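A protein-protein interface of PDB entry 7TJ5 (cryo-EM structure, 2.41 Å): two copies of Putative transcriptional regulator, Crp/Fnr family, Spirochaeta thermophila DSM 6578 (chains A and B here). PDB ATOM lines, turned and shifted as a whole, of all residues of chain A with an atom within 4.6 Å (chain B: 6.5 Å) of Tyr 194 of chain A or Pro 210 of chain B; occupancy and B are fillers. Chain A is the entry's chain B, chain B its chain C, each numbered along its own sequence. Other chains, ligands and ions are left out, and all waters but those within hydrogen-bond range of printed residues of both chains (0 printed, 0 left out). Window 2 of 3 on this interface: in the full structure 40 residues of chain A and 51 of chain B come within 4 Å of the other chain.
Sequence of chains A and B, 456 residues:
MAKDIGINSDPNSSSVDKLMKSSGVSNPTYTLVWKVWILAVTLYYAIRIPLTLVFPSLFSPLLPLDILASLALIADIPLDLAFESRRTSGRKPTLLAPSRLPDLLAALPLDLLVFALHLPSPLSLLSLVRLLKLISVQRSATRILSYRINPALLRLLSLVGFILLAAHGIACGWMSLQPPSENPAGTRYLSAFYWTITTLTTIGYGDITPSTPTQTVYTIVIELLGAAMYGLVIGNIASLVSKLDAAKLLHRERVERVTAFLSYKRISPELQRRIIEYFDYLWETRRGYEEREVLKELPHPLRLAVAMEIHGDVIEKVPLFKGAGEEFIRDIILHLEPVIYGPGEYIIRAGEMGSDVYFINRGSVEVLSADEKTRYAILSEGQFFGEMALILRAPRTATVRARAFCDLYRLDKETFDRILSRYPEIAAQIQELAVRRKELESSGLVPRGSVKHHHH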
ATOM      1  N   LEU A 190      -7.891  30.616 -34.281  1.00  0.00           N
ATOM      2  CA  LEU A 190      -7.391  29.901 -33.116  1.00  0.00           C
ATOM      3  C   LEU A 190      -7.153  30.858 -31.956  1.00  0.00           C
ATOM      4  O   LEU A 190      -7.375  30.492 -30.797  1.00  0.00           O
ATOM      5  CB  LEU A 190      -6.103  29.157 -33.459  1.00  0.00           C
ATOM      6  CG  LEU A 190      -5.629  28.118 -32.439  1.00  0.00           C
ATOM      7  CD1 LEU A 190      -6.740  27.146 -32.092  1.00  0.00           C
ATOM      8  CD2 LEU A 190      -4.405  27.381 -32.959  1.00  0.00           C
ATOM      9  N   SER A 191      -6.898  32.132 -32.260  1.00  0.00           N
ATOM     10  CA  SER A 191      -6.729  33.126 -31.208  1.00  0.00           C
ATOM     11  C   SER A 191      -8.075  33.553 -30.643  1.00  0.00           C
ATOM     12  O   SER A 191      -8.224  33.675 -29.421  1.00  0.00           O
ATOM     13  CB  SER A 191      -5.962  34.338 -31.740  1.00  0.00           C
ATOM     14  OG  SER A 191      -4.635  33.987 -32.084  1.00  0.00           O
ATOM     15  N   ALA A 192      -9.068  33.779 -31.509  1.00  0.00           N
ATOM     16  CA  ALA A 192     -10.382  34.167 -31.007  1.00  0.00           C
ATOM     17  C   ALA A 192     -11.004  33.030 -30.199  1.00  0.00           C
ATOM     18  O   ALA A 192     -11.619  33.269 -29.152  1.00  0.00           O
ATOM     19  CB  ALA A 192     -11.291  34.571 -32.165  1.00  0.00           C
ATOM     20  N   PHE A 193     -10.848  31.790 -30.669  1.00  0.00           N
ATOM     21  CA  PHE A 193     -11.369  30.636 -29.947  1.00  0.00           C
ATOM     22  C   PHE A 193     -10.638  30.433 -28.626  1.00  0.00           C
ATOM     23  O   PHE A 193     -11.259  30.075 -27.619  1.00  0.00           O
ATOM     24  CB  PHE A 193     -11.273  29.381 -30.814  1.00  0.00           C
ATOM     25  CG  PHE A 193     -12.236  28.300 -30.419  1.00  0.00           C
ATOM     26  CD1 PHE A 193     -13.570  28.377 -30.782  1.00  0.00           C
ATOM     27  CD2 PHE A 193     -11.811  27.212 -29.679  1.00  0.00           C
ATOM     28  CE1 PHE A 193     -14.460  27.385 -30.418  1.00  0.00           C
ATOM     29  CE2 PHE A 193     -12.695  26.216 -29.311  1.00  0.00           C
ATOM     30  CZ  PHE A 193     -14.022  26.305 -29.682  1.00  0.00           C
ATOM     31  N   TYR A 194      -9.323  30.668 -28.604  1.00  0.00           N
ATOM     32  CA  TYR A 194      -8.581  30.597 -27.351  1.00  0.00           C
ATOM     33  C   TYR A 194      -9.083  31.638 -26.357  1.00  0.00           C
ATOM     34  O   TYR A 194      -9.299  31.328 -25.178  1.00  0.00           O
ATOM     35  CB  TYR A 194      -7.091  30.778 -27.642  1.00  0.00           C
ATOM     36  CG  TYR A 194      -6.204  30.956 -26.434  1.00  0.00           C
ATOM     37  CD1 TYR A 194      -6.257  30.072 -25.364  1.00  0.00           C
ATOM     38  CD2 TYR A 194      -5.290  31.998 -26.379  1.00  0.00           C
ATOM     39  CE1 TYR A 194      -5.436  30.234 -24.267  1.00  0.00           C
ATOM     40  CE2 TYR A 194      -4.465  32.166 -25.289  1.00  0.00           C
ATOM     41  CZ  TYR A 194      -4.542  31.282 -24.236  1.00  0.00           C
ATOM     42  OH  TYR A 194      -3.718  31.454 -23.151  1.00  0.00           O
ATOM     43  N   TRP A 195      -9.308  32.870 -26.825  1.00  0.00           N
ATOM     44  CA  TRP A 195      -9.818  33.916 -25.944  1.00  0.00           C
ATOM     45  C   TRP A 195     -11.203  33.574 -25.407  1.00  0.00           C
ATOM     46  O   TRP A 195     -11.470  33.744 -24.210  1.00  0.00           O
ATOM     47  CB  TRP A 195      -9.855  35.260 -26.674  1.00  0.00           C
ATOM     48  CG  TRP A 195     -10.561  36.330 -25.890  1.00  0.00           C
ATOM     49  CD1 TRP A 195     -10.020  37.132 -24.929  1.00  0.00           C
ATOM     50  CD2 TRP A 195     -11.943  36.702 -25.988  1.00  0.00           C
ATOM     51  NE1 TRP A 195     -10.973  37.981 -24.427  1.00  0.00           N
ATOM     52  CE2 TRP A 195     -12.163  37.737 -25.058  1.00  0.00           C
ATOM     53  CE3 TRP A 195     -13.013  36.260 -26.771  1.00  0.00           C
ATOM     54  CZ2 TRP A 195     -13.410  38.337 -24.892  1.00  0.00           C
ATOM     55  CZ3 TRP A 195     -14.250  36.856 -26.603  1.00  0.00           C
ATOM     56  CH2 TRP A 195     -14.437  37.885 -25.671  1.00  0.00           C
ATOM     57  N   THR A 196     -12.099  33.083 -26.269  1.00  0.00           N
ATOM     58  CA  THR A 196     -13.454  32.809 -25.797  1.00  0.00           C
ATOM     59  C   THR A 196     -13.499  31.593 -24.877  1.00  0.00           C
ATOM     60  O   THR A 196     -14.297  31.574 -23.936  1.00  0.00           O
ATOM     61  CB  THR A 196     -14.438  32.650 -26.967  1.00  0.00           C
ATOM     62  OG1 THR A 196     -15.760  32.452 -26.452  1.00  0.00           O
ATOM     63  CG2 THR A 196     -14.096  31.475 -27.838  1.00  0.00           C
ATOM     64  N   ILE A 197     -12.654  30.584 -25.102  1.00  0.00           N
ATOM     65  CA  ILE A 197     -12.616  29.451 -24.182  1.00  0.00           C
ATOM     66  C   ILE A 197     -12.025  29.876 -22.842  1.00  0.00           C
ATOM     67  O   ILE A 197     -12.487  29.438 -21.781  1.00  0.00           O
ATOM     68  CB  ILE A 197     -11.848  28.273 -24.812  1.00  0.00           C
ATOM     69  CG1 ILE A 197     -12.639  27.695 -25.987  1.00  0.00           C
ATOM     70  CG2 ILE A 197     -11.580  27.181 -23.787  1.00  0.00           C
ATOM     71  CD1 ILE A 197     -14.050  27.281 -25.632  1.00  0.00           C
ATOM     72  N   THR A 198     -11.012  30.747 -22.863  1.00  0.00           N
ATOM     73  CA  THR A 198     -10.449  31.254 -21.615  1.00  0.00           C
ATOM     74  C   THR A 198     -11.471  32.082 -20.840  1.00  0.00           C
ATOM     75  O   THR A 198     -11.511  32.034 -19.606  1.00  0.00           O
ATOM     76  CB  THR A 198      -9.197  32.083 -21.908  1.00  0.00           C
ATOM     77  OG1 THR A 198      -8.346  31.363 -22.808  1.00  0.00           O
ATOM     78  CG2 THR A 198      -8.433  32.365 -20.629  1.00  0.00           C
ATOM     79  N   TYR A 205      -6.603  33.967 -18.328  1.00  0.00           N
ATOM     80  CA  TYR A 205      -5.152  34.123 -18.342  1.00  0.00           C
ATOM     81  C   TYR A 205      -4.749  35.590 -18.416  1.00  0.00           C
ATOM     82  O   TYR A 205      -3.844  36.030 -17.698  1.00  0.00           O
ATOM     83  CB  TYR A 205      -4.548  33.351 -19.514  1.00  0.00           C
ATOM     84  CG  TYR A 205      -4.476  31.855 -19.319  1.00  0.00           C
ATOM     85  CD1 TYR A 205      -3.946  31.310 -18.156  1.00  0.00           C
ATOM     86  CD2 TYR A 205      -4.934  30.988 -20.300  1.00  0.00           C
ATOM     87  CE1 TYR A 205      -3.875  29.943 -17.980  1.00  0.00           C
ATOM     88  CE2 TYR A 205      -4.866  29.621 -20.133  1.00  0.00           C
ATOM     89  CZ  TYR A 205      -4.337  29.104 -18.972  1.00  0.00           C
ATOM     90  OH  TYR A 205      -4.272  27.743 -18.805  1.00  0.00           O
ATOM     91  N   ASP A 207      -3.646  37.195 -21.266  1.00  0.00           N
ATOM     92  CA  ASP A 207      -2.717  37.530 -22.339  1.00  0.00           C
ATOM     93  C   ASP A 207      -3.431  38.185 -23.518  1.00  0.00           C
ATOM     94  O   ASP A 207      -2.832  39.006 -24.220  1.00  0.00           O
ATOM     95  CB  ASP A 207      -1.949  36.285 -22.786  1.00  0.00           C
ATOM     96  CG  ASP A 207      -2.856  35.113 -23.087  1.00  0.00           C
ATOM     97  OD1 ASP A 207      -3.816  34.887 -22.324  1.00  0.00           O
ATOM     98  OD2 ASP A 207      -2.595  34.403 -24.081  1.00  0.00           O
ATOM     99  N   ILE A 208      -4.697  37.840 -23.743  1.00  0.00           N
ATOM    100  CA  ILE A 208      -5.540  38.476 -24.750  1.00  0.00           C
ATOM    101  C   ILE A 208      -6.623  39.259 -24.020  1.00  0.00           C
ATOM    102  O   ILE A 208      -7.454  38.669 -23.317  1.00  0.00           O
ATOM    103  CB  ILE A 208      -6.155  37.447 -25.710  1.00  0.00           C
ATOM    104  CG1 ILE A 208      -5.073  36.534 -26.287  1.00  0.00           C
ATOM    105  CG2 ILE A 208      -6.928  38.146 -26.819  1.00  0.00           C
ATOM    106  CD1 ILE A 208      -5.597  35.509 -27.262  1.00  0.00           C
ATOM    107  N   TRP B 174       2.223  18.711 -21.514  1.00  0.00           N
ATOM    108  CA  TRP B 174       2.643  20.096 -21.695  1.00  0.00           C
ATOM    109  C   TRP B 174       4.158  20.199 -21.812  1.00  0.00           C
ATOM    110  O   TRP B 174       4.671  20.996 -22.605  1.00  0.00           O
ATOM    111  CB  TRP B 174       2.126  20.951 -20.536  1.00  0.00           C
ATOM    112  CG  TRP B 174       2.661  22.354 -20.502  1.00  0.00           C
ATOM    113  CD1 TRP B 174       3.737  22.805 -19.799  1.00  0.00           C
ATOM    114  CD2 TRP B 174       2.126  23.492 -21.189  1.00  0.00           C
ATOM    115  NE1 TRP B 174       3.914  24.149 -20.011  1.00  0.00           N
ATOM    116  CE2 TRP B 174       2.936  24.596 -20.860  1.00  0.00           C
ATOM    117  CE3 TRP B 174       1.044  23.684 -22.054  1.00  0.00           C
ATOM    118  CZ2 TRP B 174       2.700  25.873 -21.365  1.00  0.00           C
ATOM    119  CZ3 TRP B 174       0.811  24.952 -22.554  1.00  0.00           C
ATOM    120  CH2 TRP B 174       1.634  26.029 -22.208  1.00  0.00           C
ATOM    121  N   TRP B 195       1.591  25.055 -14.177  1.00  0.00           N
ATOM    122  CA  TRP B 195       0.677  25.504 -15.223  1.00  0.00           C
ATOM    123  C   TRP B 195      -0.609  24.684 -15.238  1.00  0.00           C
ATOM    124  O   TRP B 195      -1.707  25.244 -15.345  1.00  0.00           O
ATOM    125  CB  TRP B 195       1.357  25.438 -16.592  1.00  0.00           C
ATOM    126  CG  TRP B 195       0.405  25.690 -17.729  1.00  0.00           C
ATOM    127  CD1 TRP B 195       0.033  26.901 -18.229  1.00  0.00           C
ATOM    128  CD2 TRP B 195      -0.308  24.706 -18.490  1.00  0.00           C
ATOM    129  NE1 TRP B 195      -0.861  26.736 -19.257  1.00  0.00           N
ATOM    130  CE2 TRP B 195      -1.090  25.397 -19.436  1.00  0.00           C
ATOM    131  CE3 TRP B 195      -0.362  23.309 -18.462  1.00  0.00           C
ATOM    132  CZ2 TRP B 195      -1.913  24.740 -20.347  1.00  0.00           C
ATOM    133  CZ3 TRP B 195      -1.181  22.659 -19.367  1.00  0.00           C
ATOM    134  CH2 TRP B 195      -1.945  23.374 -20.298  1.00  0.00           C
ATOM    135  N   ILE B 208       2.328  31.801 -17.244  1.00  0.00           N
ATOM    136  CA  ILE B 208       2.684  30.759 -18.202  1.00  0.00           C
ATOM    137  C   ILE B 208       1.525  30.611 -19.178  1.00  0.00           C
ATOM    138  O   ILE B 208       0.416  30.232 -18.779  1.00  0.00           O
ATOM    139  CB  ILE B 208       2.991  29.425 -17.504  1.00  0.00           C
ATOM    140  CG1 ILE B 208       4.015  29.625 -16.387  1.00  0.00           C
ATOM    141  CG2 ILE B 208       3.476  28.394 -18.513  1.00  0.00           C
ATOM    142  CD1 ILE B 208       4.389  28.352 -15.669  1.00  0.00           C
ATOM    143  N   THR B 209       1.771  30.909 -20.449  1.00  0.00           N
ATOM    144  CA  THR B 209       0.731  30.930 -21.466  1.00  0.00           C
ATOM    145  C   THR B 209       1.236  30.277 -22.743  1.00  0.00           C
ATOM    146  O   THR B 209       2.447  30.139 -22.946  1.00  0.00           O
ATOM    147  CB  THR B 209       0.265  32.364 -21.777  1.00  0.00           C
ATOM    148  OG1 THR B 209       1.376  33.151 -22.225  1.00  0.00           O
ATOM    149  CG2 THR B 209      -0.394  33.013 -20.571  1.00  0.00           C
ATOM    150  N   PRO B 210       0.320  29.838 -23.613  1.00  0.00           N
ATOM    151  CA  PRO B 210       0.711  29.301 -24.921  1.00  0.00           C
ATOM    152  C   PRO B 210       1.522  30.266 -25.772  1.00  0.00           C
ATOM    153  O   PRO B 210       1.363  31.487 -25.696  1.00  0.00           O
ATOM    154  CB  PRO B 210      -0.639  29.025 -25.581  1.00  0.00           C
ATOM    155  CG  PRO B 210      -1.459  28.602 -24.462  1.00  0.00           C
ATOM    156  CD  PRO B 210      -1.093  29.525 -23.327  1.00  0.00           C
ATOM    157  N   SER B 211       2.401  29.694 -26.593  1.00  0.00           N
ATOM    158  CA  SER B 211       3.247  30.466 -27.493  1.00  0.00           C
ATOM    159  C   SER B 211       3.164  30.000 -28.940  1.00  0.00           C
ATOM    160  O   SER B 211       3.476  30.791 -29.837  1.00  0.00           O
ATOM    161  CB  SER B 211       4.713  30.416 -27.040  1.00  0.00           C
ATOM    162  OG  SER B 211       4.923  31.232 -25.902  1.00  0.00           O
ATOM    163  N   THR B 212       2.762  28.759 -29.196  1.00  0.00           N
ATOM    164  CA  THR B 212       2.650  28.163 -30.517  1.00  0.00           C
ATOM    165  C   THR B 212       1.212  27.713 -30.752  1.00  0.00           C
ATOM    166  O   THR B 212       0.451  27.532 -29.795  1.00  0.00           O
ATOM    167  CB  THR B 212       3.602  26.966 -30.670  1.00  0.00           C
ATOM    168  OG1 THR B 212       3.077  25.839 -29.961  1.00  0.00           O
ATOM    169  CG2 THR B 212       4.983  27.303 -30.127  1.00  0.00           C
ATOM    170  N   GLN B 215       0.465  24.555 -28.883  1.00  0.00           N
ATOM    171  CA  GLN B 215       0.275  24.874 -27.473  1.00  0.00           C
ATOM    172  C   GLN B 215      -1.110  25.453 -27.229  1.00  0.00           C
ATOM    173  O   GLN B 215      -1.754  25.136 -26.225  1.00  0.00           O
ATOM    174  CB  GLN B 215       1.349  25.856 -27.001  1.00  0.00           C
ATOM    175  CG  GLN B 215       2.733  25.255 -26.838  1.00  0.00           C
ATOM    176  CD  GLN B 215       3.769  26.275 -26.424  1.00  0.00           C
ATOM    177  OE1 GLN B 215       3.456  27.447 -26.224  1.00  0.00           O
ATOM    178  NE2 GLN B 215       5.013  25.836 -26.298  1.00  0.00           N
ATOM    179  N   THR B 216      -1.588  26.297 -28.146  1.00  0.00           N
ATOM    180  CA  THR B 216      -2.903  26.907 -27.988  1.00  0.00           C
ATOM    181  C   THR B 216      -4.019  25.870 -28.067  1.00  0.00           C
ATOM    182  O   THR B 216      -4.959  25.904 -27.264  1.00  0.00           O
ATOM    183  CB  THR B 216      -3.100  27.989 -29.051  1.00  0.00           C
ATOM    184  OG1 THR B 216      -1.975  28.876 -29.045  1.00  0.00           O
ATOM    185  CG2 THR B 216      -4.361  28.784 -28.778  1.00  0.00           C
ATOM    186  N   VAL B 217      -3.931  24.938 -29.019  1.00  0.00           N
ATOM    187  CA  VAL B 217      -4.947  23.891 -29.132  1.00  0.00           C
ATOM    188  C   VAL B 217      -4.933  22.994 -27.899  1.00  0.00           C
ATOM    189  O   VAL B 217      -5.991  22.662 -27.335  1.00  0.00           O
ATOM    190  CB  VAL B 217      -4.731  23.079 -30.424  1.00  0.00           C
ATOM    191  CG1 VAL B 217      -5.667  21.878 -30.468  1.00  0.00           C
ATOM    192  CG2 VAL B 217      -4.932  23.959 -31.644  1.00  0.00           C
ATOM    193  N   THR B 219      -3.934  23.814 -24.917  1.00  0.00           N
ATOM    194  CA  THR B 219      -4.454  24.596 -23.803  1.00  0.00           C
ATOM    195  C   THR B 219      -5.970  24.715 -23.859  1.00  0.00           C
ATOM    196  O   THR B 219      -6.630  24.673 -22.822  1.00  0.00           O
ATOM    197  CB  THR B 219      -3.791  25.970 -23.787  1.00  0.00           C
ATOM    198  OG1 THR B 219      -2.381  25.794 -23.615  1.00  0.00           O
ATOM    199  CG2 THR B 219      -4.330  26.829 -22.652  1.00  0.00           C
ATOM    200  N   ILE B 220      -6.542  24.877 -25.055  1.00  0.00           N
ATOM    201  CA  ILE B 220      -7.998  24.934 -25.177  1.00  0.00           C
ATOM    202  C   ILE B 220      -8.620  23.627 -24.694  1.00  0.00           C
ATOM    203  O   ILE B 220      -9.595  23.621 -23.924  1.00  0.00           O
ATOM    204  CB  ILE B 220      -8.406  25.252 -26.628  1.00  0.00           C
ATOM    205  CG1 ILE B 220      -8.072  26.704 -26.974  1.00  0.00           C
ATOM    206  CG2 ILE B 220      -9.886  24.982 -26.846  1.00  0.00           C
ATOM    207  CD1 ILE B 220      -8.186  27.015 -28.450  1.00  0.00           C
ATOM    208  N   GLU B 223      -8.279  23.437 -20.919  1.00  0.00           N
ATOM    209  CA  GLU B 223      -9.233  24.337 -20.276  1.00  0.00           C
ATOM    210  C   GLU B 223     -10.622  23.721 -20.231  1.00  0.00           C
ATOM    211  O   GLU B 223     -11.319  23.809 -19.211  1.00  0.00           O
ATOM    212  CB  GLU B 223      -9.276  25.679 -21.009  1.00  0.00           C
ATOM    213  CG  GLU B 223      -8.058  26.559 -20.801  1.00  0.00           C
ATOM    214  CD  GLU B 223      -8.140  27.857 -21.578  1.00  0.00           C
ATOM    215  OE1 GLU B 223      -8.134  27.808 -22.826  1.00  0.00           O
ATOM    216  OE2 GLU B 223      -8.207  28.930 -20.945  1.00  0.00           O
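The side-chain hydroxyl (OG1) of Thr 198 of chain A lies within hydrogen-bond range of the backbone carbonyl oxygen (O) of Tyr 194 of chain A. The side-chain hydroxyl (OH) of Tyr 194 of chain A lies close to the side-chain carboxylate (OD2) of Asp 207 of chain A (3.3 Å). The side-chain hydroxyl of Thr 216 of chain B is in hydrogen-bond range of the backbone carbonyl oxygen of Thr 212 of chain B, at 2.9 Å. O of Gln 215 of chain B lies within hydrogen-bond range of OG1 of Thr 219 of chain B.
The side-chain hydroxyl of Thr 198 of chain A sits at hydrogen-bond distance from the side-chain carboxylate of Glu 223 of chain B.
Of the printed residues of chain B, Tyr 194 of chain A touches Pro 210 (3.3 Å), Thr 216 (3.6 Å), Thr 219 (3.9 Å), Ile 220 (3.8 Å) and Glu 223 (3.9 Å). Of chain A, only Tyr 194 (3.3 Å) comes within 4 Å of Pro 210 of chain B. Printed residues of chain B within 4 Å of Thr 198 of chain A: Glu 223 (3.1 Å). Printed residues of chain A within 4 Å of Thr 219 of chain B: Tyr 194 and Tyr 205. Ser 191 of chain A touches none of the printed residues of chain B. Gln 215 of chain B touches none of the printed residues of chain A. The nearest residue of chain B that does not touch Tyr 194 of chain A is Thr 209 of chain B (4.3 Å). The nearest printed residue of chain A that does not touch Pro 210 of chain B is Tyr 205 of chain A (4.9 Å). The nearest printed residue of chain A that does not touch Trp 195 of chain B is Tyr 194 of chain A (6.8 Å).
Among the printed residues, merely in contact across the chains: Leu 190 of chain A with Thr 216 of chain B, Leu 190 of chain A with Val 217 of chain B, Leu 190 of chain A with Ile 220 of chain B, Phe 193 of chain A with Ile 220 of chain B, Tyr 194 of chain A with Pro 210 of chain B, Tyr 194 of chain A with Thr 216 of chain B, Tyr 194 of chain A with Thr 219 of chain B, Tyr 194 of chain A with Ile 220 of chain B, Tyr 194 of chain A with Glu 223 of chain B, Ile 197 of chain A with Ile 220 of chain B, Ile 197 of chain A with Glu 223 of chain B, Tyr 205 of chain A with Trp 195 of chain B, Tyr 205 of chain A with Thr 219 of chain B and Tyr 205 of chain A with Glu 223 of chain B.
2 positions are printed for both chains.
Of the 13 printed residues of chain B, 7 touch a printed residue of chain A. Printed residues of chain B that touch a printed residue of chain A: Trp 195, Pro 210, Thr 216, Val 217, Thr 219, Ile 220 and Glu 223. Among the printed residues, no Asp or Glu carboxylate lies within 4 Å of a Lys or Arg side-chain nitrogen of the other chain.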
